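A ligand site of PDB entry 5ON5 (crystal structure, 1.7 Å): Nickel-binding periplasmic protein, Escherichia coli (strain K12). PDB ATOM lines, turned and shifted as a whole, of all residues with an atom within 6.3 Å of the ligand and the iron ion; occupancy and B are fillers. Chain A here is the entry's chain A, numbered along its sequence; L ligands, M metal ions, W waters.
NE1 of Trp 100 sits at hydrogen-bond distance from OH of Tyr 22 (2.8 Å).
The side-chain hydroxyl of Tyr 22 lies within hydrogen-bond range of a ring nitrogen (ND1) of His 98, at 2.7 Å.
No residue comes within 4 Å of the iron ion.
The nearest printed residue that does not touch the iron ion is Arg 137 (4.3 Å).
An oxygen (O2) of the ligand binds the iron ion, at 1.9 Å.
The iron ion is bound by N1 of the ligand (2.1 Å).
O3 of the ligand is bound to the iron ion (2.2 Å).
An oxygen (O5) of the ligand is bound to the iron ion, 2.2 Å away.
A nitrogen (N2) of the ligand is bound to the iron ion, 2.3 Å away.
Water W3 is bound to the iron ion, at 2.4 Å.
The iron ion has six donor atoms within binding distance.
Water W4 lies within hydrogen-bond range of OH of Tyr 402 (2.7 Å), O of Arg 137 (2.8 Å) and O4 of the ligand (2.8 Å).
NE of Arg 137 is in salt-bridge range of O4 of the ligand (2.8 Å).
S1 of the ligand lies close to OG1 of Thr 23 (3.7 Å).
Residues that only touch the ligand: Tyr 22, Met 27, Arg 97, Trp 100, Trp 398, Tyr 402, His 416 and Thr 490.
Hydrophobic or aromatic side chains that line the ligand: Tyr 22, Met 27, Trp 100, Trp 398, Tyr 402 and His 416.
Ten residues have an atom within 4 Å of the ligand: Tyr 22, Thr 23, Met 27, Arg 97, Trp 100, Arg 137, Trp 398, Tyr 402, His 416 and Thr 490.
Along chain A the residues within 4 Å of the ligand span positions 22 to 490.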
ATOM      1  N   TYR A  22      -7.612   1.577  22.492  1.00  0.00           N
ATOM      2  CA  TYR A  22      -8.622   0.619  22.037  1.00  0.00           C
ATOM      3  C   TYR A  22      -9.907   0.807  22.845  1.00  0.00           C
ATOM      4  O   TYR A  22     -10.358   1.931  22.987  1.00  0.00           O
ATOM      5  CB  TYR A  22      -8.047  -0.804  22.121  1.00  0.00           C
ATOM      6  CG  TYR A  22      -6.777  -0.931  21.297  1.00  0.00           C
ATOM      7  CD1 TYR A  22      -6.836  -1.242  19.945  1.00  0.00           C
ATOM      8  CD2 TYR A  22      -5.523  -0.697  21.859  1.00  0.00           C
ATOM      9  CE1 TYR A  22      -5.688  -1.332  19.170  1.00  0.00           C
ATOM     10  CE2 TYR A  22      -4.356  -0.797  21.096  1.00  0.00           C
ATOM     11  CZ  TYR A  22      -4.450  -1.114  19.754  1.00  0.00           C
ATOM     12  OH  TYR A  22      -3.319  -1.221  18.977  1.00  0.00           O
ATOM     13  N   THR A  23     -10.471  -0.281  23.374  1.00  0.00           N
ATOM     14  CA  THR A  23     -11.672  -0.205  24.211  1.00  0.00           C
ATOM     15  C   THR A  23     -11.530   0.869  25.279  1.00  0.00           C
ATOM     16  O   THR A  23     -10.503   0.945  25.952  1.00  0.00           O
ATOM     17  CB  THR A  23     -11.951  -1.573  24.900  1.00  0.00           C
ATOM     18  OG1 THR A  23     -11.572  -2.638  24.029  1.00  0.00           O
ATOM     19  CG2 THR A  23     -13.419  -1.702  25.265  1.00  0.00           C
ATOM     20  N   MET A  27     -13.852   1.929  16.679  1.00  0.00           N
ATOM     21  CA  MET A  27     -13.001   2.124  15.508  1.00  0.00           C
ATOM     22  C   MET A  27     -13.634   2.979  14.408  1.00  0.00           C
ATOM     23  O   MET A  27     -12.964   3.827  13.827  1.00  0.00           O
ATOM     24  CB  MET A  27     -12.594   0.770  14.915  1.00  0.00           C
ATOM     25  CG  MET A  27     -11.970  -0.164  15.931  1.00  0.00           C
ATOM     26  SD  MET A  27     -11.519  -1.778  15.259  1.00  0.00           S
ATOM     27  CE  MET A  27     -10.162  -1.232  14.242  1.00  0.00           C
ATOM     28  N   ARG A  97       1.297  -2.409  24.331  1.00  0.00           N
ATOM     29  CA  ARG A  97      -0.138  -2.574  24.117  1.00  0.00           C
ATOM     30  C   ARG A  97      -0.460  -2.879  22.654  1.00  0.00           C
ATOM     31  O   ARG A  97      -1.573  -3.295  22.331  1.00  0.00           O
ATOM     32  CB  ARG A  97      -0.897  -1.312  24.567  1.00  0.00           C
ATOM     33  CG  ARG A  97      -2.404  -1.550  24.766  1.00  0.00           C
ATOM     34  CD  ARG A  97      -3.160  -0.293  25.178  1.00  0.00           C
ATOM     35  NE  ARG A  97      -4.601  -0.436  24.940  1.00  0.00           N
ATOM     36  CZ  ARG A  97      -5.543   0.308  25.530  1.00  0.00           C
ATOM     37  NH1 ARG A  97      -5.200   1.226  26.418  1.00  0.00           N
ATOM     38  NH2 ARG A  97      -6.819   0.117  25.247  1.00  0.00           N
ATOM     39  N   HIS A  98       0.513  -2.687  21.772  1.00  0.00           N
ATOM     40  CA  HIS A  98       0.277  -2.886  20.345  1.00  0.00           C
ATOM     41  C   HIS A  98       0.930  -4.153  19.805  1.00  0.00           C
ATOM     42  O   HIS A  98       1.091  -4.306  18.600  1.00  0.00           O
ATOM     43  CB  HIS A  98       0.761  -1.664  19.553  1.00  0.00           C
ATOM     44  CG  HIS A  98       0.238  -0.363  20.073  1.00  0.00           C
ATOM     45  ND1 HIS A  98      -1.097  -0.036  20.050  1.00  0.00           N
ATOM     46  CD2 HIS A  98       0.875   0.682  20.649  1.00  0.00           C
ATOM     47  CE1 HIS A  98      -1.269   1.164  20.579  1.00  0.00           C
ATOM     48  NE2 HIS A  98      -0.083   1.621  20.945  1.00  0.00           N
ATOM     49  N   ALA A  99       1.301  -5.062  20.701  1.00  0.00           N
ATOM     50  CA  ALA A  99       1.998  -6.298  20.321  1.00  0.00           C
ATOM     51  C   ALA A  99       1.285  -7.102  19.238  1.00  0.00           C
ATOM     52  O   ALA A  99       1.919  -7.757  18.408  1.00  0.00           O
ATOM     53  CB  ALA A  99       2.230  -7.160  21.550  1.00  0.00           C
ATOM     54  N   TRP A 100      -0.048  -7.051  19.258  1.00  0.00           N
ATOM     55  CA  TRP A 100      -0.854  -7.771  18.270  1.00  0.00           C
ATOM     56  C   TRP A 100      -0.551  -7.322  16.845  1.00  0.00           C
ATOM     57  O   TRP A 100      -0.727  -8.079  15.891  1.00  0.00           O
ATOM     58  CB  TRP A 100      -2.338  -7.586  18.553  1.00  0.00           C
ATOM     59  CG  TRP A 100      -2.800  -6.199  18.264  1.00  0.00           C
ATOM     60  CD1 TRP A 100      -2.761  -5.136  19.111  1.00  0.00           C
ATOM     61  CD2 TRP A 100      -3.364  -5.714  17.040  1.00  0.00           C
ATOM     62  NE1 TRP A 100      -3.258  -4.021  18.491  1.00  0.00           N
ATOM     63  CE2 TRP A 100      -3.635  -4.344  17.216  1.00  0.00           C
ATOM     64  CE3 TRP A 100      -3.653  -6.307  15.809  1.00  0.00           C
ATOM     65  CZ2 TRP A 100      -4.194  -3.557  16.215  1.00  0.00           C
ATOM     66  CZ3 TRP A 100      -4.209  -5.528  14.803  1.00  0.00           C
ATOM     67  CH2 TRP A 100      -4.468  -4.169  15.012  1.00  0.00           C
ATOM     68  N   PRO A 136      -7.601   1.781  10.971  1.00  0.00           N
ATOM     69  CA  PRO A 136      -8.299   2.775  11.802  1.00  0.00           C
ATOM     70  C   PRO A 136      -7.455   3.263  12.984  1.00  0.00           C
ATOM     71  O   PRO A 136      -7.521   4.439  13.349  1.00  0.00           O
ATOM     72  CB  PRO A 136      -9.543   2.014  12.287  1.00  0.00           C
ATOM     73  CG  PRO A 136      -9.809   1.040  11.185  1.00  0.00           C
ATOM     74  CD  PRO A 136      -8.452   0.608  10.692  1.00  0.00           C
ATOM     75  N   ARG A 137      -6.683   2.352  13.579  1.00  0.00           N
ATOM     76  CA  ARG A 137      -5.829   2.659  14.731  1.00  0.00           C
ATOM     77  C   ARG A 137      -4.705   1.630  14.768  1.00  0.00           C
ATOM     78  O   ARG A 137      -4.875   0.528  14.244  1.00  0.00           O
ATOM     79  CB  ARG A 137      -6.649   2.635  16.031  1.00  0.00           C
ATOM     80  CG  ARG A 137      -7.273   1.275  16.354  1.00  0.00           C
ATOM     81  CD  ARG A 137      -8.382   1.419  17.382  1.00  0.00           C
ATOM     82  NE  ARG A 137      -8.927   0.129  17.812  1.00  0.00           N
ATOM     83  CZ  ARG A 137     -10.003   0.000  18.586  1.00  0.00           C
ATOM     84  NH1 ARG A 137     -10.656   1.081  18.982  1.00  0.00           N
ATOM     85  NH2 ARG A 137     -10.436  -1.211  18.935  1.00  0.00           N
ATOM     86  N   PRO A 138      -3.563   1.963  15.382  1.00  0.00           N
ATOM     87  CA  PRO A 138      -3.257   3.182  16.127  1.00  0.00           C
ATOM     88  C   PRO A 138      -2.527   4.290  15.368  1.00  0.00           C
ATOM     89  O   PRO A 138      -2.282   5.329  15.957  1.00  0.00           O
ATOM     90  CB  PRO A 138      -2.348   2.659  17.252  1.00  0.00           C
ATOM     91  CG  PRO A 138      -1.548   1.616  16.549  1.00  0.00           C
ATOM     92  CD  PRO A 138      -2.512   0.945  15.585  1.00  0.00           C
ATOM     93  N   GLU A 247     -16.137 -11.253   6.424  1.00  0.00           N
ATOM     94  CA  GLU A 247     -15.274 -11.995   7.339  1.00  0.00           C
ATOM     95  C   GLU A 247     -15.922 -13.308   7.765  1.00  0.00           C
ATOM     96  O   GLU A 247     -17.092 -13.557   7.488  1.00  0.00           O
ATOM     97  CB  GLU A 247     -14.939 -11.131   8.573  1.00  0.00           C
ATOM     98  CG  GLU A 247     -16.145 -10.868   9.480  1.00  0.00           C
ATOM     99  CD  GLU A 247     -16.072  -9.546  10.224  1.00  0.00           C
ATOM    100  OE1 GLU A 247     -15.254  -8.674   9.848  1.00  0.00           O
ATOM    101  OE2 GLU A 247     -16.842  -9.382  11.197  1.00  0.00           O
ATOM    102  N   GLN A 385     -10.802 -16.354  26.504  1.00  0.00           N
ATOM    103  CA  GLN A 385     -10.061 -16.348  25.255  1.00  0.00           C
ATOM    104  C   GLN A 385      -8.564 -16.145  25.459  1.00  0.00           C
ATOM    105  O   GLN A 385      -7.741 -16.806  24.828  1.00  0.00           O
ATOM    106  CB  GLN A 385     -10.588 -15.264  24.314  1.00  0.00           C
ATOM    107  CG  GLN A 385     -11.930 -15.578  23.707  1.00  0.00           C
ATOM    108  CD  GLN A 385     -12.327 -14.566  22.652  1.00  0.00           C
ATOM    109  OE1 GLN A 385     -11.761 -13.484  22.569  1.00  0.00           O
ATOM    110  NE2 GLN A 385     -13.309 -14.922  21.817  1.00  0.00           N
ATOM    111  N   THR A 397     -12.893 -13.744  12.177  1.00  0.00           N
ATOM    112  CA  THR A 397     -11.750 -13.066  11.596  1.00  0.00           C
ATOM    113  C   THR A 397     -12.071 -11.579  11.495  1.00  0.00           C
ATOM    114  O   THR A 397     -13.099 -11.125  11.990  1.00  0.00           O
ATOM    115  CB  THR A 397     -11.352 -13.645  10.217  1.00  0.00           C
ATOM    116  OG1 THR A 397     -12.376 -13.391   9.251  1.00  0.00           O
ATOM    117  CG2 THR A 397     -11.084 -15.141  10.323  1.00  0.00           C
ATOM    118  N   TRP A 398     -11.183 -10.829  10.866  1.00  0.00           N
ATOM    119  CA  TRP A 398     -11.186  -9.374  11.065  1.00  0.00           C
ATOM    120  C   TRP A 398     -11.561  -8.564   9.840  1.00  0.00           C
ATOM    121  O   TRP A 398     -11.720  -7.333   9.928  1.00  0.00           O
ATOM    122  CB  TRP A 398      -9.806  -8.949  11.568  1.00  0.00           C
ATOM    123  CG  TRP A 398      -9.479  -9.471  12.958  1.00  0.00           C
ATOM    124  CD1 TRP A 398     -10.352 -10.035  13.840  1.00  0.00           C
ATOM    125  CD2 TRP A 398      -8.197  -9.444  13.608  1.00  0.00           C
ATOM    126  NE1 TRP A 398      -9.688 -10.361  15.004  1.00  0.00           N
ATOM    127  CE2 TRP A 398      -8.370 -10.021  14.887  1.00  0.00           C
ATOM    128  CE3 TRP A 398      -6.925  -8.996  13.235  1.00  0.00           C
ATOM    129  CZ2 TRP A 398      -7.310 -10.160  15.787  1.00  0.00           C
ATOM    130  CZ3 TRP A 398      -5.884  -9.138  14.128  1.00  0.00           C
ATOM    131  CH2 TRP A 398      -6.086  -9.706  15.393  1.00  0.00           C
ATOM    132  N   GLY A 399     -11.706  -9.230   8.698  1.00  0.00           N
ATOM    133  CA  GLY A 399     -12.050  -8.551   7.452  1.00  0.00           C
ATOM    134  C   GLY A 399     -10.885  -7.801   6.835  1.00  0.00           C
ATOM    135  O   GLY A 399      -9.790  -7.763   7.397  1.00  0.00           O
ATOM    136  N   TYR A 402      -7.216  -6.669   7.302  1.00  0.00           N
ATOM    137  CA  TYR A 402      -6.563  -7.535   8.294  1.00  0.00           C
ATOM    138  C   TYR A 402      -6.380  -8.968   7.823  1.00  0.00           C
ATOM    139  O   TYR A 402      -5.406  -9.636   8.184  1.00  0.00           O
ATOM    140  CB  TYR A 402      -7.351  -7.558   9.592  1.00  0.00           C
ATOM    141  CG  TYR A 402      -7.567  -6.220  10.260  1.00  0.00           C
ATOM    142  CD1 TYR A 402      -8.694  -5.443   9.970  1.00  0.00           C
ATOM    143  CD2 TYR A 402      -6.680  -5.744  11.210  1.00  0.00           C
ATOM    144  CE1 TYR A 402      -8.905  -4.223  10.596  1.00  0.00           C
ATOM    145  CE2 TYR A 402      -6.882  -4.522  11.839  1.00  0.00           C
ATOM    146  CZ  TYR A 402      -7.985  -3.773  11.527  1.00  0.00           C
ATOM    147  OH  TYR A 402      -8.184  -2.559  12.152  1.00  0.00           O
ATOM    148  N   HIS A 416      -4.050 -14.115  22.983  1.00  0.00           N
ATOM    149  CA  HIS A 416      -5.125 -14.106  21.981  1.00  0.00           C
ATOM    150  C   HIS A 416      -5.733 -15.503  21.860  1.00  0.00           C
ATOM    151  O   HIS A 416      -5.046 -16.505  22.050  1.00  0.00           O
ATOM    152  CB  HIS A 416      -4.615 -13.657  20.609  1.00  0.00           C
ATOM    153  CG  HIS A 416      -4.692 -12.182  20.375  1.00  0.00           C
ATOM    154  ND1 HIS A 416      -5.530 -11.626  19.428  1.00  0.00           N
ATOM    155  CD2 HIS A 416      -4.023 -11.148  20.928  1.00  0.00           C
ATOM    156  CE1 HIS A 416      -5.382 -10.313  19.430  1.00  0.00           C
ATOM    157  NE2 HIS A 416      -4.472  -9.993  20.332  1.00  0.00           N
ATOM    158  N   THR A 490     -14.417  -2.444   9.099  1.00  0.00           N
ATOM    159  CA  THR A 490     -14.867  -1.871  10.354  1.00  0.00           C
ATOM    160  C   THR A 490     -15.164  -0.371  10.268  1.00  0.00           C
ATOM    161  O   THR A 490     -15.546   0.253  11.250  1.00  0.00           O
ATOM    162  CB  THR A 490     -13.839  -2.119  11.456  1.00  0.00           C
ATOM    163  OG1 THR A 490     -14.418  -1.809  12.727  1.00  0.00           O
ATOM    164  CG2 THR A 490     -12.581  -1.276  11.222  1.00  0.00           C
HETATM  165  C1  LIG L   1     -14.467  -4.716  15.437  1.00  0.00           C
HETATM  166  O1  LIG L   1     -13.286  -5.052  16.160  1.00  0.00           O
HETATM  167  C2  LIG L   1     -12.265  -5.424  15.344  1.00  0.00           C
HETATM  168  C3  LIG L   1     -11.106  -5.848  15.964  1.00  0.00           C
HETATM  169  O2  LIG L   1     -11.064  -5.857  17.317  1.00  0.00           O
HETATM  170  C4  LIG L   1     -12.338  -5.407  13.953  1.00  0.00           C
HETATM  171  C5  LIG L   1     -11.224  -5.811  13.224  1.00  0.00           C
HETATM  172  C6  LIG L   1     -10.062  -6.229  13.860  1.00  0.00           C
HETATM  173  C7  LIG L   1      -9.986  -6.256  15.247  1.00  0.00           C
HETATM  174  C8  LIG L   1      -8.822  -6.687  15.888  1.00  0.00           C
HETATM  175  N1  LIG L   1      -8.339  -5.702  16.862  1.00  0.00           N
HETATM  176  C9  LIG L   1      -7.992  -4.482  16.117  1.00  0.00           C
HETATM  177  C10 LIG L   1      -8.267  -3.244  16.972  1.00  0.00           C
HETATM  178  O3  LIG L   1      -8.926  -3.414  18.018  1.00  0.00           O
HETATM  179  O4  LIG L   1      -7.819  -2.157  16.554  1.00  0.00           O
HETATM  180  C11 LIG L   1      -7.118  -6.273  17.472  1.00  0.00           C
HETATM  181  C12 LIG L   1      -6.746  -5.601  18.793  1.00  0.00           C
HETATM  182  N2  LIG L   1      -7.811  -5.681  19.810  1.00  0.00           N
HETATM  183  C13 LIG L   1      -7.817  -6.981  20.514  1.00  0.00           C
HETATM  184  C14 LIG L   1      -8.737  -7.997  19.812  1.00  0.00           C
HETATM  185  O5  LIG L   1      -9.703  -7.544  19.152  1.00  0.00           O
HETATM  186  O6  LIG L   1      -8.460  -9.205  19.955  1.00  0.00           O
HETATM  187  C15 LIG L   1      -7.814  -4.548  20.770  1.00  0.00           C
HETATM  188  C16 LIG L   1      -6.822  -4.530  21.778  1.00  0.00           C
HETATM  189  C17 LIG L   1      -5.479  -4.268  21.481  1.00  0.00           C
HETATM  190  C18 LIG L   1      -4.509  -4.231  22.482  1.00  0.00           C
HETATM  191  C19 LIG L   1      -4.870  -4.450  23.801  1.00  0.00           C
HETATM  192  C20 LIG L   1      -6.200  -4.692  24.113  1.00  0.00           C
HETATM  193  C21 LIG L   1      -7.170  -4.728  23.111  1.00  0.00           C
HETATM  194  S1  LIG L   1      -8.856  -5.056  23.555  1.00  0.00           S
HETATM  195  C22 LIG L   1      -8.809  -4.680  25.297  1.00  0.00           C
HETATM  196 FE    FE M   1      -9.640  -5.416  18.467  1.00  0.00          FE
HETATM  197  O   HOH W   1     -13.053  -3.626  18.471  1.00  0.00           O
HETATM  198  O   HOH W   2     -12.289  -8.221  18.231  1.00  0.00           O
HETATM  199  O   HOH W   3     -11.059  -4.627  20.178  1.00  0.00           O
HETATM  200  O   HOH W   4      -6.534  -1.689  14.103  1.00  0.00           O
